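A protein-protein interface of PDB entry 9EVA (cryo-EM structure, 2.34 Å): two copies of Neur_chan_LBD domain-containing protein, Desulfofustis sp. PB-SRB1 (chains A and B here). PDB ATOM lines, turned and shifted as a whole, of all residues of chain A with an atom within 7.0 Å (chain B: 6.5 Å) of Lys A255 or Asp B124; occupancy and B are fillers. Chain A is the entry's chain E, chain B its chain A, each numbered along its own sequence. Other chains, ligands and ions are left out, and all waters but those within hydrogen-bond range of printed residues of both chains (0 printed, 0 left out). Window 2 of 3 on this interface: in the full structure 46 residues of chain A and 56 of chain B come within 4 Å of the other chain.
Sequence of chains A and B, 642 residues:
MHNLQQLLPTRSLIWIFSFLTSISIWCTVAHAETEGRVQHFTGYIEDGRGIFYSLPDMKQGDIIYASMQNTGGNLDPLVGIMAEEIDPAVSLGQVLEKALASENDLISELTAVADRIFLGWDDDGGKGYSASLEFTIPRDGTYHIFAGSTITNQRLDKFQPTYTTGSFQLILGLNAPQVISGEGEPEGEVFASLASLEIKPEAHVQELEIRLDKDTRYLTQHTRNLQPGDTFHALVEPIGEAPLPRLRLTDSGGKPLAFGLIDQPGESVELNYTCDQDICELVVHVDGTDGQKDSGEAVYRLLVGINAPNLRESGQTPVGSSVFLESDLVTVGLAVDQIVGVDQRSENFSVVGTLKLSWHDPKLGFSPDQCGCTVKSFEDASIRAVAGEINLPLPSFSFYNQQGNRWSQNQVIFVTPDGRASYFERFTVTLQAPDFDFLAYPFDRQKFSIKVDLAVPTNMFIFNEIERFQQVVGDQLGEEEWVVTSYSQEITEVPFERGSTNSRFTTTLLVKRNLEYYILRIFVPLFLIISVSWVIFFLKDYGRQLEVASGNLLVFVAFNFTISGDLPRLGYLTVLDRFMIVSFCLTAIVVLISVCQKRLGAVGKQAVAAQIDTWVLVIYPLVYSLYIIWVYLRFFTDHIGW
Asn B153 touches Gly A253. CA of Gln B154 touches O of Gly A253, 3.6 Å away. Lys A255 touches Tyr B129 (NZ to CD1, 3.6 Å). CG2 of Thr B152 touches CE of Lys A255 (3.5 Å). O of Asn B153 touches N of Lys A255, 3.7 Å away. CG of Pro A256 touches CD1 of Ile B107, 3.7 Å away.
The side-chain carboxylate (OD2) of Asp B124 is in salt-bridge range of the side-chain amino group (NZ) of Lys A255, 2.6 Å away. OD2 of Asp B76 is in salt-bridge range of NZ of Lys A255 (3.5 Å). ND2 of Asn B153 is in hydrogen-bond range of O of Gly A254 (3.4 Å). OH of Tyr B129 lies within hydrogen-bond range of OD2 of Asp A251, 2.9 Å away.
O of Asp B76 lies within hydrogen-bond range of N of Thr B150, 3.4 Å away. The backbone NH (N) of Gly A254 sits at hydrogen-bond distance from the side-chain carboxylate (OD1) of Asp A251 (3.2 Å). The side-chain carboxylate (OD1) of Asp A251 lies within hydrogen-bond range of the backbone NH (N) of Lys A255, at 2.6 Å. The side-chain carboxylate (OD1) of Asp A251 sits close to the backbone NH (N) of Gly A253, at 3.5 Å.
Of the printed residues of chain B, Lys A255 touches Asp B76, Asp B124, Tyr B129, Thr B152 and Asn B153. Asp B124 touches just one residue of chain A: Lys A255. Of the printed residues of chain A, Gln B154 touches Gly A253. Of the printed residues of chain A, Thr B152 touches Lys A255. Of the printed residues of chain A, Tyr B129 touches Asp A251 (2.9 Å) and Lys A255 (3.6 Å). Lys B127 touches none of the printed residues of chain A. The nearest residue of chain B that does not touch Lys A255 is Asp B123 (4.4 Å). The nearest residue of chain A that does not touch Asp B124 is Gln A277 (5.8 Å). The nearest printed residue of chain A that does not touch Thr B152 is Pro A256 (5.0 Å).
No position is printed for both chains. Of the 10 pairs that touch across the chains among the printed residues, none has its exchanged pair printed and touching as well.
Of the 11 printed residues of chain A, 5 touch a printed residue of chain B. Hydrophobic or aromatic side chains of chain A that line the printed part of chain B: Pro A256. Along chain A the printed residues that touch a printed residue of chain B span positions 251 to 256. Hydrophobic or aromatic side chains of chain B within 4 Å of the printed part of chain A: Ile B107 and Tyr B129.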
ATOM      1  N   LEU A 249      -8.431  24.121  39.894  1.00  0.00           N
ATOM      2  CA  LEU A 249      -9.804  24.590  39.773  1.00  0.00           C
ATOM      3  C   LEU A 249     -10.299  24.354  38.354  1.00  0.00           C
ATOM      4  O   LEU A 249      -9.624  24.725  37.390  1.00  0.00           O
ATOM      5  CB  LEU A 249      -9.907  26.078  40.125  1.00  0.00           C
ATOM      6  CG  LEU A 249     -11.282  26.726  39.974  1.00  0.00           C
ATOM      7  CD1 LEU A 249     -12.272  26.082  40.921  1.00  0.00           C
ATOM      8  CD2 LEU A 249     -11.199  28.220  40.217  1.00  0.00           C
ATOM      9  N   THR A 250     -11.476  23.741  38.230  1.00  0.00           N
ATOM     10  CA  THR A 250     -12.095  23.467  36.941  1.00  0.00           C
ATOM     11  C   THR A 250     -13.572  23.828  36.993  1.00  0.00           C
ATOM     12  O   THR A 250     -14.174  23.916  38.066  1.00  0.00           O
ATOM     13  CB  THR A 250     -11.951  21.992  36.530  1.00  0.00           C
ATOM     14  OG1 THR A 250     -12.572  21.155  37.512  1.00  0.00           O
ATOM     15  CG2 THR A 250     -10.488  21.605  36.393  1.00  0.00           C
ATOM     16  N   ASP A 251     -14.154  24.037  35.815  1.00  0.00           N
ATOM     17  CA  ASP A 251     -15.590  24.250  35.722  1.00  0.00           C
ATOM     18  C   ASP A 251     -16.322  22.911  35.809  1.00  0.00           C
ATOM     19  O   ASP A 251     -15.731  21.858  36.063  1.00  0.00           O
ATOM     20  CB  ASP A 251     -15.937  24.994  34.433  1.00  0.00           C
ATOM     21  CG  ASP A 251     -15.677  24.169  33.192  1.00  0.00           C
ATOM     22  OD1 ASP A 251     -14.815  23.269  33.240  1.00  0.00           O
ATOM     23  OD2 ASP A 251     -16.335  24.423  32.164  1.00  0.00           O
ATOM     24  N   SER A 252     -17.634  22.950  35.590  1.00  0.00           N
ATOM     25  CA  SER A 252     -18.466  21.760  35.708  1.00  0.00           C
ATOM     26  C   SER A 252     -18.224  20.742  34.602  1.00  0.00           C
ATOM     27  O   SER A 252     -18.648  19.591  34.744  1.00  0.00           O
ATOM     28  CB  SER A 252     -19.944  22.151  35.724  1.00  0.00           C
ATOM     29  OG  SER A 252     -20.240  22.970  36.839  1.00  0.00           O
ATOM     30  N   GLY A 253     -17.567  21.128  33.512  1.00  0.00           N
ATOM     31  CA  GLY A 253     -17.276  20.196  32.443  1.00  0.00           C
ATOM     32  C   GLY A 253     -15.895  19.588  32.540  1.00  0.00           C
ATOM     33  O   GLY A 253     -15.578  18.632  31.825  1.00  0.00           O
ATOM     34  N   GLY A 254     -15.063  20.128  33.422  1.00  0.00           N
ATOM     35  CA  GLY A 254     -13.702  19.665  33.581  1.00  0.00           C
ATOM     36  C   GLY A 254     -12.634  20.536  32.959  1.00  0.00           C
ATOM     37  O   GLY A 254     -11.452  20.190  33.053  1.00  0.00           O
ATOM     38  N   LYS A 255     -13.004  21.648  32.339  1.00  0.00           N
ATOM     39  CA  LYS A 255     -12.018  22.530  31.724  1.00  0.00           C
ATOM     40  C   LYS A 255     -11.172  23.198  32.800  1.00  0.00           C
ATOM     41  O   LYS A 255     -11.720  23.852  33.695  1.00  0.00           O
ATOM     42  CB  LYS A 255     -12.718  23.587  30.876  1.00  0.00           C
ATOM     43  CG  LYS A 255     -12.426  23.511  29.394  1.00  0.00           C
ATOM     44  CD  LYS A 255     -11.166  24.271  29.048  1.00  0.00           C
ATOM     45  CE  LYS A 255     -10.973  24.350  27.549  1.00  0.00           C
ATOM     46  NZ  LYS A 255     -12.181  24.871  26.865  1.00  0.00           N
ATOM     47  N   PRO A 256      -9.848  23.062  32.754  1.00  0.00           N
ATOM     48  CA  PRO A 256      -9.009  23.693  33.779  1.00  0.00           C
ATOM     49  C   PRO A 256      -9.077  25.210  33.702  1.00  0.00           C
ATOM     50  O   PRO A 256      -9.202  25.791  32.622  1.00  0.00           O
ATOM     51  CB  PRO A 256      -7.603  23.175  33.457  1.00  0.00           C
ATOM     52  CG  PRO A 256      -7.661  22.797  32.018  1.00  0.00           C
ATOM     53  CD  PRO A 256      -9.054  22.307  31.772  1.00  0.00           C
ATOM     54  N   LEU A 257      -8.995  25.845  34.862  1.00  0.00           N
ATOM     55  CA  LEU A 257      -9.065  27.298  34.960  1.00  0.00           C
ATOM     56  C   LEU A 257      -7.904  27.901  35.734  1.00  0.00           C
ATOM     57  O   LEU A 257      -7.480  29.015  35.419  1.00  0.00           O
ATOM     58  CB  LEU A 257     -10.394  27.717  35.603  1.00  0.00           C
ATOM     59  CG  LEU A 257     -11.657  27.422  34.792  1.00  0.00           C
ATOM     60  CD1 LEU A 257     -12.899  27.785  35.580  1.00  0.00           C
ATOM     61  CD2 LEU A 257     -11.631  28.161  33.466  1.00  0.00           C
ATOM     62  N   ALA A 258      -7.380  27.202  36.737  1.00  0.00           N
ATOM     63  CA  ALA A 258      -6.251  27.703  37.508  1.00  0.00           C
ATOM     64  C   ALA A 258      -5.534  26.533  38.162  1.00  0.00           C
ATOM     65  O   ALA A 258      -6.096  25.447  38.324  1.00  0.00           O
ATOM     66  CB  ALA A 258      -6.697  28.721  38.562  1.00  0.00           C
ATOM     67  N   GLN A 277     -17.569  34.703  32.427  1.00  0.00           N
ATOM     68  CA  GLN A 277     -18.840  34.334  31.822  1.00  0.00           C
ATOM     69  C   GLN A 277     -20.011  34.887  32.631  1.00  0.00           C
ATOM     70  O   GLN A 277     -19.856  35.388  33.747  1.00  0.00           O
ATOM     71  CB  GLN A 277     -18.959  32.815  31.695  1.00  0.00           C
ATOM     72  CG  GLN A 277     -18.152  32.208  30.556  1.00  0.00           C
ATOM     73  CD  GLN A 277     -16.687  32.033  30.903  1.00  0.00           C
ATOM     74  OE1 GLN A 277     -16.343  31.349  31.867  1.00  0.00           O
ATOM     75  NE2 GLN A 277     -15.814  32.651  30.116  1.00  0.00           N
ATOM     76  N   ASP B  76     -13.349  19.829  20.890  1.00  0.00           N
ATOM     77  CA  ASP B  76     -13.123  21.152  21.460  1.00  0.00           C
ATOM     78  C   ASP B  76     -12.339  21.996  20.462  1.00  0.00           C
ATOM     79  O   ASP B  76     -11.122  21.801  20.317  1.00  0.00           O
ATOM     80  CB  ASP B  76     -12.367  21.043  22.783  1.00  0.00           C
ATOM     81  CG  ASP B  76     -12.626  22.215  23.703  1.00  0.00           C
ATOM     82  OD1 ASP B  76     -12.909  23.319  23.197  1.00  0.00           O
ATOM     83  OD2 ASP B  76     -12.552  22.030  24.934  1.00  0.00           O
ATOM     84  N   PRO B  77     -12.977  22.933  19.762  1.00  0.00           N
ATOM     85  CA  PRO B  77     -12.311  23.615  18.643  1.00  0.00           C
ATOM     86  C   PRO B  77     -11.112  24.455  19.064  1.00  0.00           C
ATOM     87  O   PRO B  77     -11.052  24.995  20.171  1.00  0.00           O
ATOM     88  CB  PRO B  77     -13.421  24.498  18.063  1.00  0.00           C
ATOM     89  CG  PRO B  77     -14.687  23.847  18.497  1.00  0.00           C
ATOM     90  CD  PRO B  77     -14.402  23.279  19.848  1.00  0.00           C
ATOM     91  N   ILE B 107      -2.335  24.921  31.249  1.00  0.00           N
ATOM     92  CA  ILE B 107      -2.782  26.201  30.689  1.00  0.00           C
ATOM     93  C   ILE B 107      -1.633  27.135  30.533  1.00  0.00           C
ATOM     94  O   ILE B 107      -1.695  28.069  29.747  1.00  0.00           O
ATOM     95  CB  ILE B 107      -3.864  26.872  31.518  1.00  0.00           C
ATOM     96  CG1 ILE B 107      -5.074  25.948  31.685  1.00  0.00           C
ATOM     97  CG2 ILE B 107      -4.298  28.167  30.856  1.00  0.00           C
ATOM     98  CD1 ILE B 107      -5.705  25.529  30.377  1.00  0.00           C
ATOM     99  N   ASP B 122      -7.134  31.396  19.100  1.00  0.00           N
ATOM    100  CA  ASP B 122      -8.202  31.551  20.077  1.00  0.00           C
ATOM    101  C   ASP B 122      -8.734  30.175  20.445  1.00  0.00           C
ATOM    102  O   ASP B 122      -8.868  29.309  19.579  1.00  0.00           O
ATOM    103  CB  ASP B 122      -9.338  32.428  19.544  1.00  0.00           C
ATOM    104  CG  ASP B 122     -10.447  32.618  20.560  1.00  0.00           C
ATOM    105  OD1 ASP B 122     -10.204  33.289  21.585  1.00  0.00           O
ATOM    106  OD2 ASP B 122     -11.559  32.098  20.337  1.00  0.00           O
ATOM    107  N   ASP B 123      -9.034  29.984  21.730  1.00  0.00           N
ATOM    108  CA  ASP B 123      -9.524  28.704  22.231  1.00  0.00           C
ATOM    109  C   ASP B 123     -11.027  28.736  22.486  1.00  0.00           C
ATOM    110  O   ASP B 123     -11.766  27.951  21.888  1.00  0.00           O
ATOM    111  CB  ASP B 123      -8.762  28.317  23.499  1.00  0.00           C
ATOM    112  CG  ASP B 123      -8.850  26.836  23.805  1.00  0.00           C
ATOM    113  OD1 ASP B 123      -9.827  26.188  23.375  1.00  0.00           O
ATOM    114  OD2 ASP B 123      -7.937  26.316  24.476  1.00  0.00           O
ATOM    115  N   ASP B 124     -11.507  29.626  23.352  1.00  0.00           N
ATOM    116  CA  ASP B 124     -12.876  29.585  23.854  1.00  0.00           C
ATOM    117  C   ASP B 124     -13.552  30.948  23.774  1.00  0.00           C
ATOM    118  O   ASP B 124     -14.340  31.319  24.646  1.00  0.00           O
ATOM    119  CB  ASP B 124     -12.905  29.069  25.290  1.00  0.00           C
ATOM    120  CG  ASP B 124     -12.356  27.666  25.416  1.00  0.00           C
ATOM    121  OD1 ASP B 124     -12.631  26.840  24.523  1.00  0.00           O
ATOM    122  OD2 ASP B 124     -11.645  27.390  26.405  1.00  0.00           O
ATOM    123  N   GLY B 125     -13.269  31.706  22.719  1.00  0.00           N
ATOM    124  CA  GLY B 125     -13.803  33.051  22.619  1.00  0.00           C
ATOM    125  C   GLY B 125     -15.265  33.151  22.249  1.00  0.00           C
ATOM    126  O   GLY B 125     -15.831  34.245  22.322  1.00  0.00           O
ATOM    127  N   GLY B 126     -15.897  32.042  21.862  1.00  0.00           N
ATOM    128  CA  GLY B 126     -17.264  32.044  21.416  1.00  0.00           C
ATOM    129  C   GLY B 126     -18.220  31.467  22.439  1.00  0.00           C
ATOM    130  O   GLY B 126     -17.912  31.358  23.633  1.00  0.00           O
ATOM    131  N   LYS B 127     -19.403  31.089  21.961  1.00  0.00           N
ATOM    132  CA  LYS B 127     -20.438  30.526  22.822  1.00  0.00           C
ATOM    133  C   LYS B 127     -20.025  29.117  23.226  1.00  0.00           C
ATOM    134  O   LYS B 127     -19.953  28.217  22.383  1.00  0.00           O
ATOM    135  CB  LYS B 127     -21.787  30.517  22.109  1.00  0.00           C
ATOM    136  CG  LYS B 127     -22.319  31.899  21.767  1.00  0.00           C
ATOM    137  CD  LYS B 127     -23.686  31.815  21.106  1.00  0.00           C
ATOM    138  CE  LYS B 127     -24.237  33.198  20.797  1.00  0.00           C
ATOM    139  NZ  LYS B 127     -25.580  33.129  20.155  1.00  0.00           N
ATOM    140  N   GLY B 128     -19.756  28.925  24.512  1.00  0.00           N
ATOM    141  CA  GLY B 128     -19.276  27.647  24.990  1.00  0.00           C
ATOM    142  C   GLY B 128     -17.791  27.492  24.751  1.00  0.00           C
ATOM    143  O   GLY B 128     -17.008  28.386  25.081  1.00  0.00           O
ATOM    144  N   TYR B 129     -17.391  26.363  24.169  1.00  0.00           N
ATOM    145  CA  TYR B 129     -15.994  26.075  23.882  1.00  0.00           C
ATOM    146  C   TYR B 129     -15.607  26.438  22.453  1.00  0.00           C
ATOM    147  O   TYR B 129     -14.502  26.104  22.013  1.00  0.00           O
ATOM    148  CB  TYR B 129     -15.695  24.601  24.156  1.00  0.00           C
ATOM    149  CG  TYR B 129     -15.861  24.195  25.603  1.00  0.00           C
ATOM    150  CD1 TYR B 129     -15.734  25.122  26.625  1.00  0.00           C
ATOM    151  CD2 TYR B 129     -16.146  22.882  25.946  1.00  0.00           C
ATOM    152  CE1 TYR B 129     -15.886  24.753  27.946  1.00  0.00           C
ATOM    153  CE2 TYR B 129     -16.299  22.505  27.263  1.00  0.00           C
ATOM    154  CZ  TYR B 129     -16.169  23.443  28.258  1.00  0.00           C
ATOM    155  OH  TYR B 129     -16.320  23.069  29.571  1.00  0.00           O
ATOM    156  N   SER B 130     -16.487  27.121  21.728  1.00  0.00           N
ATOM    157  CA  SER B 130     -16.218  27.496  20.348  1.00  0.00           C
ATOM    158  C   SER B 130     -15.232  28.657  20.285  1.00  0.00           C
ATOM    159  O   SER B 130     -15.178  29.495  21.187  1.00  0.00           O
ATOM    160  CB  SER B 130     -17.517  27.873  19.639  1.00  0.00           C
ATOM    161  OG  SER B 130     -18.145  28.970  20.277  1.00  0.00           O
ATOM    162  N   ALA B 131     -14.454  28.699  19.210  1.00  0.00           N
ATOM    163  CA  ALA B 131     -13.417  29.702  19.024  1.00  0.00           C
ATOM    164  C   ALA B 131     -13.870  30.796  18.064  1.00  0.00           C
ATOM    165  O   ALA B 131     -14.699  30.570  17.179  1.00  0.00           O
ATOM    166  CB  ALA B 131     -12.130  29.061  18.501  1.00  0.00           C
ATOM    167  N   SER B 132     -13.314  31.992  18.254  1.00  0.00           N
ATOM    168  CA  SER B 132     -13.553  33.121  17.367  1.00  0.00           C
ATOM    169  C   SER B 132     -12.303  33.986  17.342  1.00  0.00           C
ATOM    170  O   SER B 132     -11.722  34.267  18.392  1.00  0.00           O
ATOM    171  CB  SER B 132     -14.768  33.937  17.814  1.00  0.00           C
ATOM    172  OG  SER B 132     -14.620  34.372  19.152  1.00  0.00           O
ATOM    173  N   THR B 150      -7.832  21.228  20.759  1.00  0.00           N
ATOM    174  CA  THR B 150      -6.974  21.621  21.865  1.00  0.00           C
ATOM    175  C   THR B 150      -6.798  20.462  22.845  1.00  0.00           C
ATOM    176  O   THR B 150      -7.357  19.376  22.679  1.00  0.00           O
ATOM    177  CB  THR B 150      -7.552  22.838  22.584  1.00  0.00           C
ATOM    178  OG1 THR B 150      -6.763  23.128  23.744  1.00  0.00           O
ATOM    179  CG2 THR B 150      -8.981  22.573  23.005  1.00  0.00           C
ATOM    180  N   ILE B 151      -6.001  20.705  23.881  1.00  0.00           N
ATOM    181  CA  ILE B 151      -5.755  19.730  24.938  1.00  0.00           C
ATOM    182  C   ILE B 151      -6.592  20.119  26.148  1.00  0.00           C
ATOM    183  O   ILE B 151      -6.421  21.211  26.703  1.00  0.00           O
ATOM    184  CB  ILE B 151      -4.264  19.658  25.296  1.00  0.00           C
ATOM    185  CG1 ILE B 151      -3.441  19.259  24.073  1.00  0.00           C
ATOM    186  CG2 ILE B 151      -4.038  18.680  26.436  1.00  0.00           C
ATOM    187  CD1 ILE B 151      -1.954  19.215  24.331  1.00  0.00           C
ATOM    188  N   THR B 152      -7.486  19.225  26.567  1.00  0.00           N
ATOM    189  CA  THR B 152      -8.436  19.529  27.630  1.00  0.00           C
ATOM    190  C   THR B 152      -8.624  18.313  28.525  1.00  0.00           C
ATOM    191  O   THR B 152      -8.230  17.196  28.185  1.00  0.00           O
ATOM    192  CB  THR B 152      -9.799  19.962  27.074  1.00  0.00           C
ATOM    193  OG1 THR B 152     -10.296  18.960  26.181  1.00  0.00           O
ATOM    194  CG2 THR B 152      -9.692  21.282  26.337  1.00  0.00           C
ATOM    195  N   ASN B 153      -9.227  18.556  29.685  1.00  0.00           N
ATOM    196  CA  ASN B 153      -9.658  17.513  30.607  1.00  0.00           C
ATOM    197  C   ASN B 153     -11.179  17.520  30.678  1.00  0.00           C
ATOM    198  O   ASN B 153     -11.795  18.589  30.713  1.00  0.00           O
ATOM    199  CB  ASN B 153      -9.057  17.728  31.996  1.00  0.00           C
ATOM    200  CG  ASN B 153      -9.495  16.676  32.990  1.00  0.00           C
ATOM    201  OD1 ASN B 153      -9.002  15.550  32.975  1.00  0.00           O
ATOM    202  ND2 ASN B 153     -10.419  17.039  33.869  1.00  0.00           N
ATOM    203  N   GLN B 154     -11.782  16.330  30.687  1.00  0.00           N
ATOM    204  CA  GLN B 154     -13.235  16.199  30.691  1.00  0.00           C
ATOM    205  C   GLN B 154     -13.713  15.208  31.747  1.00  0.00           C
ATOM    206  O   GLN B 154     -14.711  14.517  31.542  1.00  0.00           O
ATOM    207  CB  GLN B 154     -13.746  15.782  29.314  1.00  0.00           C
ATOM    208  CG  GLN B 154     -13.487  16.791  28.216  1.00  0.00           C
ATOM    209  CD  GLN B 154     -13.824  16.254  26.841  1.00  0.00           C
ATOM    210  OE1 GLN B 154     -13.426  15.148  26.481  1.00  0.00           O
ATOM    211  NE2 GLN B 154     -14.569  17.034  26.067  1.00  0.00           N
